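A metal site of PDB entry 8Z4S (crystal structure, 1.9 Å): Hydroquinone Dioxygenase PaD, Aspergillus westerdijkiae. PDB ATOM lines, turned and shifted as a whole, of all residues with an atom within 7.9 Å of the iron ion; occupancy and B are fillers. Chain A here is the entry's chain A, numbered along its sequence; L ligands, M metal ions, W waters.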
ATOM      1  N   HIS A  61      31.772 -15.206  -8.993  1.00  0.00           N
ATOM      2  CA  HIS A  61      30.525 -15.908  -9.394  1.00  0.00           C
ATOM      3  C   HIS A  61      29.433 -14.932  -9.810  1.00  0.00           C
ATOM      4  O   HIS A  61      29.295 -13.880  -9.191  1.00  0.00           O
ATOM      5  CB  HIS A  61      30.032 -16.818  -8.242  1.00  0.00           C
ATOM      6  CG  HIS A  61      31.037 -17.821  -7.838  1.00  0.00           C
ATOM      7  ND1 HIS A  61      32.121 -17.499  -7.065  1.00  0.00           N
ATOM      8  CD2 HIS A  61      31.120 -19.152  -8.065  1.00  0.00           C
ATOM      9  CE1 HIS A  61      32.845 -18.579  -6.881  1.00  0.00           C
ATOM     10  NE2 HIS A  61      32.293 -19.572  -7.527  1.00  0.00           N
ATOM     11  N   ASN A  62      28.610 -15.380 -10.749  1.00  0.00           N
ATOM     12  CA  ASN A  62      27.354 -14.705 -11.169  1.00  0.00           C
ATOM     13  C   ASN A  62      26.324 -14.953 -10.050  1.00  0.00           C
ATOM     14  O   ASN A  62      25.909 -16.104  -9.886  1.00  0.00           O
ATOM     15  CB  ASN A  62      26.933 -15.254 -12.527  1.00  0.00           C
ATOM     16  CG  ASN A  62      25.630 -14.648 -13.018  1.00  0.00           C
ATOM     17  OD1 ASN A  62      25.146 -13.708 -12.429  1.00  0.00           O
ATOM     18  ND2 ASN A  62      25.126 -15.151 -14.140  1.00  0.00           N
ATOM     19  N   HIS A  63      25.934 -13.909  -9.345  1.00  0.00           N
ATOM     20  CA  HIS A  63      24.956 -13.959  -8.219  1.00  0.00           C
ATOM     21  C   HIS A  63      23.582 -13.523  -8.700  1.00  0.00           C
ATOM     22  O   HIS A  63      22.691 -13.340  -7.842  1.00  0.00           O
ATOM     23  CB  HIS A  63      25.381 -13.065  -7.091  1.00  0.00           C
ATOM     24  CG  HIS A  63      26.538 -13.646  -6.378  1.00  0.00           C
ATOM     25  ND1 HIS A  63      27.781 -13.714  -6.970  1.00  0.00           N
ATOM     26  CD2 HIS A  63      26.642 -14.215  -5.168  1.00  0.00           C
ATOM     27  CE1 HIS A  63      28.610 -14.267  -6.116  1.00  0.00           C
ATOM     28  NE2 HIS A  63      27.945 -14.635  -5.019  1.00  0.00           N
ATOM     29  N   HIS A  66      20.483 -15.657  -7.697  1.00  0.00           N
ATOM     30  CA  HIS A  66      20.308 -15.545  -6.223  1.00  0.00           C
ATOM     31  C   HIS A  66      19.762 -14.175  -5.820  1.00  0.00           C
ATOM     32  O   HIS A  66      18.901 -14.080  -4.929  1.00  0.00           O
ATOM     33  CB  HIS A  66      21.641 -15.694  -5.438  1.00  0.00           C
ATOM     34  CG  HIS A  66      22.520 -16.826  -5.835  1.00  0.00           C
ATOM     35  ND1 HIS A  66      23.851 -16.892  -5.440  1.00  0.00           N
ATOM     36  CD2 HIS A  66      22.290 -17.926  -6.599  1.00  0.00           C
ATOM     37  CE1 HIS A  66      24.395 -17.969  -5.952  1.00  0.00           C
ATOM     38  NE2 HIS A  66      23.471 -18.613  -6.679  1.00  0.00           N
ATOM     39  N   GLY A 163      34.591 -23.113  -4.466  1.00  0.00           N
ATOM     40  CA  GLY A 163      34.251 -21.749  -4.926  1.00  0.00           C
ATOM     41  C   GLY A 163      33.372 -21.089  -3.905  1.00  0.00           C
ATOM     42  O   GLY A 163      32.404 -20.440  -4.301  1.00  0.00           O
ATOM     43  N   TYR A 164      33.715 -21.245  -2.620  1.00  0.00           N
ATOM     44  CA  TYR A 164      32.993 -20.654  -1.475  1.00  0.00           C
ATOM     45  C   TYR A 164      31.503 -21.082  -1.506  1.00  0.00           C
ATOM     46  O   TYR A 164      30.628 -20.215  -1.322  1.00  0.00           O
ATOM     47  CB  TYR A 164      33.235 -19.137  -1.415  1.00  0.00           C
ATOM     48  CG  TYR A 164      34.710 -18.830  -1.597  1.00  0.00           C
ATOM     49  CD1 TYR A 164      35.640 -19.230  -0.649  1.00  0.00           C
ATOM     50  CD2 TYR A 164      35.189 -18.250  -2.763  1.00  0.00           C
ATOM     51  CE1 TYR A 164      37.002 -19.023  -0.842  1.00  0.00           C
ATOM     52  CE2 TYR A 164      36.539 -18.031  -2.966  1.00  0.00           C
ATOM     53  CZ  TYR A 164      37.457 -18.408  -1.997  1.00  0.00           C
ATOM     54  OH  TYR A 164      38.787 -18.180  -2.225  1.00  0.00           O
ATOM     55  N   VAL A 165      31.263 -22.373  -1.721  1.00  0.00           N
ATOM     56  CA  VAL A 165      29.962 -23.084  -1.494  1.00  0.00           C
ATOM     57  C   VAL A 165      28.857 -22.535  -2.426  1.00  0.00           C
ATOM     58  O   VAL A 165      27.668 -22.676  -2.099  1.00  0.00           O
ATOM     59  CB  VAL A 165      29.589 -23.106   0.007  1.00  0.00           C
ATOM     60  CG1 VAL A 165      30.766 -23.627   0.850  1.00  0.00           C
ATOM     61  CG2 VAL A 165      29.140 -21.798   0.595  1.00  0.00           C
ATOM     62  N   HIS A 166      29.193 -21.974  -3.588  1.00  0.00           N
ATOM     63  CA  HIS A 166      28.148 -21.404  -4.486  1.00  0.00           C
ATOM     64  C   HIS A 166      27.263 -22.535  -5.054  1.00  0.00           C
ATOM     65  O   HIS A 166      26.060 -22.241  -5.275  1.00  0.00           O
ATOM     66  CB  HIS A 166      28.734 -20.379  -5.503  1.00  0.00           C
ATOM     67  CG  HIS A 166      29.059 -19.064  -4.844  1.00  0.00           C
ATOM     68  ND1 HIS A 166      30.319 -18.777  -4.322  1.00  0.00           N
ATOM     69  CD2 HIS A 166      28.308 -17.963  -4.594  1.00  0.00           C
ATOM     70  CE1 HIS A 166      30.298 -17.581  -3.739  1.00  0.00           C
ATOM     71  NE2 HIS A 166      29.062 -17.062  -3.864  1.00  0.00           N
ATOM     72  N   ILE A 169      24.699 -23.396  -2.422  1.00  0.00           N
ATOM     73  CA  ILE A 169      23.780 -22.236  -2.357  1.00  0.00           C
ATOM     74  C   ILE A 169      22.747 -22.347  -3.501  1.00  0.00           C
ATOM     75  O   ILE A 169      21.509 -22.197  -3.248  1.00  0.00           O
ATOM     76  CB  ILE A 169      24.544 -20.888  -2.330  1.00  0.00           C
ATOM     77  CG1 ILE A 169      25.257 -20.640  -0.995  1.00  0.00           C
ATOM     78  CG2 ILE A 169      23.613 -19.720  -2.636  1.00  0.00           C
ATOM     79  CD1 ILE A 169      26.317 -19.566  -1.102  1.00  0.00           C
ATOM     80  N   PHE A 313      32.768 -10.823   4.264  1.00  0.00           N
ATOM     81  CA  PHE A 313      32.369 -11.283   2.911  1.00  0.00           C
ATOM     82  C   PHE A 313      32.450 -12.810   2.818  1.00  0.00           C
ATOM     83  O   PHE A 313      31.573 -13.445   2.206  1.00  0.00           O
ATOM     84  CB  PHE A 313      33.259 -10.660   1.831  1.00  0.00           C
ATOM     85  CG  PHE A 313      32.818 -11.049   0.457  1.00  0.00           C
ATOM     86  CD1 PHE A 313      31.695 -10.464  -0.112  1.00  0.00           C
ATOM     87  CD2 PHE A 313      33.465 -12.058  -0.249  1.00  0.00           C
ATOM     88  CE1 PHE A 313      31.256 -10.845  -1.359  1.00  0.00           C
ATOM     89  CE2 PHE A 313      33.020 -12.432  -1.501  1.00  0.00           C
ATOM     90  CZ  PHE A 313      31.902 -11.827  -2.051  1.00  0.00           C
ATOM     91  N   LEU A 316      30.076 -14.795   5.592  1.00  0.00           N
ATOM     92  CA  LEU A 316      28.608 -14.754   5.405  1.00  0.00           C
ATOM     93  C   LEU A 316      28.106 -15.817   4.435  1.00  0.00           C
ATOM     94  O   LEU A 316      26.879 -16.151   4.527  1.00  0.00           O
ATOM     95  CB  LEU A 316      28.111 -13.368   5.058  1.00  0.00           C
ATOM     96  CG  LEU A 316      28.533 -12.806   3.717  1.00  0.00           C
ATOM     97  CD1 LEU A 316      27.726 -13.437   2.591  1.00  0.00           C
ATOM     98  CD2 LEU A 316      28.374 -11.298   3.778  1.00  0.00           C
ATOM     99  N   HIS A 317      28.970 -16.455   3.656  1.00  0.00           N
ATOM    100  CA  HIS A 317      28.573 -17.609   2.826  1.00  0.00           C
ATOM    101  C   HIS A 317      28.191 -18.809   3.723  1.00  0.00           C
ATOM    102  O   HIS A 317      27.461 -19.672   3.248  1.00  0.00           O
ATOM    103  CB  HIS A 317      29.653 -17.987   1.801  1.00  0.00           C
ATOM    104  CG  HIS A 317      29.744 -16.959   0.735  1.00  0.00           C
ATOM    105  ND1 HIS A 317      30.256 -15.710   0.995  1.00  0.00           N
ATOM    106  CD2 HIS A 317      29.265 -16.925  -0.543  1.00  0.00           C
ATOM    107  CE1 HIS A 317      30.138 -14.953  -0.085  1.00  0.00           C
ATOM    108  NE2 HIS A 317      29.547 -15.672  -1.040  1.00  0.00           N
ATOM    109  N   THR A 320      24.422 -17.934   4.301  1.00  0.00           N
ATOM    110  CA  THR A 320      23.588 -18.058   3.086  1.00  0.00           C
ATOM    111  C   THR A 320      23.560 -19.511   2.599  1.00  0.00           C
ATOM    112  O   THR A 320      22.549 -19.913   2.017  1.00  0.00           O
ATOM    113  CB  THR A 320      24.038 -17.063   2.012  1.00  0.00           C
ATOM    114  OG1 THR A 320      25.377 -17.377   1.654  1.00  0.00           O
ATOM    115  CG2 THR A 320      23.955 -15.642   2.489  1.00  0.00           C
ATOM    116  N   ASP A 392      25.319  -7.084  -5.285  1.00  0.00           N
ATOM    117  CA  ASP A 392      25.101  -8.232  -6.179  1.00  0.00           C
ATOM    118  C   ASP A 392      24.223  -9.257  -5.472  1.00  0.00           C
ATOM    119  O   ASP A 392      24.058 -10.348  -6.042  1.00  0.00           O
ATOM    120  CB  ASP A 392      26.426  -8.841  -6.609  1.00  0.00           C
ATOM    121  CG  ASP A 392      27.280  -9.310  -5.442  1.00  0.00           C
ATOM    122  OD1 ASP A 392      26.915  -8.992  -4.261  1.00  0.00           O
ATOM    123  OD2 ASP A 392      28.351  -9.906  -5.736  1.00  0.00           O
ATOM    124  N   GLY A 393      23.719  -8.902  -4.302  1.00  0.00           N
ATOM    125  CA  GLY A 393      22.742  -9.715  -3.552  1.00  0.00           C
ATOM    126  C   GLY A 393      23.257 -10.272  -2.234  1.00  0.00           C
ATOM    127  O   GLY A 393      22.412 -10.779  -1.497  1.00  0.00           O
ATOM    128  N   HIS A 394      24.557 -10.136  -1.887  1.00  0.00           N
ATOM    129  CA  HIS A 394      25.073 -10.729  -0.615  1.00  0.00           C
ATOM    130  C   HIS A 394      24.304 -10.157   0.583  1.00  0.00           C
ATOM    131  O   HIS A 394      24.005 -10.920   1.550  1.00  0.00           O
ATOM    132  CB  HIS A 394      26.603 -10.544  -0.496  1.00  0.00           C
ATOM    133  CG  HIS A 394      27.333 -11.478  -1.406  1.00  0.00           C
ATOM    134  ND1 HIS A 394      27.644 -11.147  -2.726  1.00  0.00           N
ATOM    135  CD2 HIS A 394      27.690 -12.776  -1.240  1.00  0.00           C
ATOM    136  CE1 HIS A 394      28.268 -12.166  -3.299  1.00  0.00           C
ATOM    137  NE2 HIS A 394      28.283 -13.230  -2.402  1.00  0.00           N
ATOM    138  N   KCX A 397      20.677 -11.614   0.888  1.00  0.00           N
ATOM    139  CA  KCX A 397      20.698 -13.042   1.187  1.00  0.00           C
ATOM    140  CB  KCX A 397      21.650 -13.842   0.284  1.00  0.00           C
ATOM    141  CG  KCX A 397      21.300 -13.860  -1.191  1.00  0.00           C
ATOM    142  CD  KCX A 397      22.464 -14.224  -2.098  1.00  0.00           C
ATOM    143  CE  KCX A 397      23.109 -15.567  -1.772  1.00  0.00           C
ATOM    144  NZ  KCX A 397      24.425 -15.712  -2.408  1.00  0.00           N
ATOM    145  C   KCX A 397      21.105 -13.283   2.648  1.00  0.00           C
ATOM    146  O   KCX A 397      20.573 -14.207   3.272  1.00  0.00           O
ATOM    147  CX  KCX A 397      25.593 -15.874  -1.701  1.00  0.00           C
ATOM    148  OQ1 KCX A 397      26.663 -16.161  -2.423  1.00  0.00           O
ATOM    149  OQ2 KCX A 397      25.675 -15.786  -0.499  1.00  0.00           O
ATOM    150  N   HIS A 446      33.536  -5.201  -3.788  1.00  0.00           N
ATOM    151  CA  HIS A 446      32.663  -4.941  -2.619  1.00  0.00           C
ATOM    152  C   HIS A 446      33.387  -4.012  -1.680  1.00  0.00           C
ATOM    153  O   HIS A 446      34.570  -4.232  -1.459  1.00  0.00           O
ATOM    154  CB  HIS A 446      32.315  -6.246  -1.893  1.00  0.00           C
ATOM    155  CG  HIS A 446      31.242  -7.064  -2.542  1.00  0.00           C
ATOM    156  ND1 HIS A 446      29.927  -6.860  -2.252  1.00  0.00           N
ATOM    157  CD2 HIS A 446      31.287  -8.046  -3.441  1.00  0.00           C
ATOM    158  CE1 HIS A 446      29.211  -7.708  -2.922  1.00  0.00           C
ATOM    159  NE2 HIS A 446      29.983  -8.459  -3.652  1.00  0.00           N
HETATM  160  C1  LIG L   1      34.188 -15.635  -4.973  1.00  0.00           C
HETATM  161  C2  LIG L   1      33.928 -14.262  -5.139  1.00  0.00           C
HETATM  162  C3  LIG L   1      34.824 -13.254  -4.759  1.00  0.00           C
HETATM  163  C4  LIG L   1      36.096 -13.529  -4.137  1.00  0.00           C
HETATM  164  C5  LIG L   1      34.446 -11.923  -5.017  1.00  0.00           C
HETATM  165  O1  LIG L   1      35.312 -10.974  -4.596  1.00  0.00           O
HETATM  166  C6  LIG L   1      33.230 -11.549  -5.621  1.00  0.00           C
HETATM  167  C7  LIG L   1      32.870 -10.207  -5.885  1.00  0.00           C
HETATM  168  C8  LIG L   1      32.350 -12.552  -6.053  1.00  0.00           C
HETATM  169  C9  LIG L   1      32.721 -13.881  -5.764  1.00  0.00           C
HETATM  170  O2  LIG L   1      31.944 -14.883  -6.099  1.00  0.00           O
HETATM  171 FE    FE M   1      28.649 -15.248  -2.983  1.00  0.00          FE
HETATM  172  O   HOH W   1      30.839 -14.574  -3.605  1.00  0.00           O
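The backbone NH (N) of His 61 is in hydrogen-bond range of an oxygen (O2) of the ligand. A ring nitrogen (ND1) of His 61 lies within hydrogen-bond range of an oxygen (O2) of the ligand (2.8 Å).
The side-chain hydroxyl (OG1) of Thr 320 lies close to the backbone carbonyl oxygen (O) of His 317 (3.5 Å). OQ2 of KCX 397 is in hydrogen-bond range of the side-chain hydroxyl of Thr 320, at 2.7 Å. A ring nitrogen (ND1) of His 166 sits at hydrogen-bond distance from the backbone carbonyl oxygen (O) of Tyr 164, at 3.3 Å. ND1 of His 166 sits at hydrogen-bond distance from O of Gly 163, 2.7 Å away. ND1 of His 63 lies within hydrogen-bond range of O of His 61, 2.7 Å away. ND1 of His 66 lies within hydrogen-bond range of NZ of KCX 397 (3.3 Å). The side-chain carboxylate (OD1) of Asp 392 lies within hydrogen-bond range of a ring nitrogen (ND1) of His 394 (2.7 Å). A ring nitrogen (ND1) of His 317 is in hydrogen-bond range of the backbone carbonyl oxygen of Phe 313, 2.9 Å away.
Five residues have an atom within 4 Å of the iron ion: His 63, His 166, His 317, His 394 and KCX 397.
The iron ion is bound by a ring nitrogen (NE2) of His 166 (2.1 Å), a ring nitrogen (NE2) of His 394 (2.1 Å), a ring nitrogen (NE2) of His 317 (2.2 Å), a ring nitrogen (NE2) of His 63 (2.2 Å), OQ1 of KCX 397 (2.3 Å) and water W1 (2.4 Å). The iron ion has six donor atoms within binding distance.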
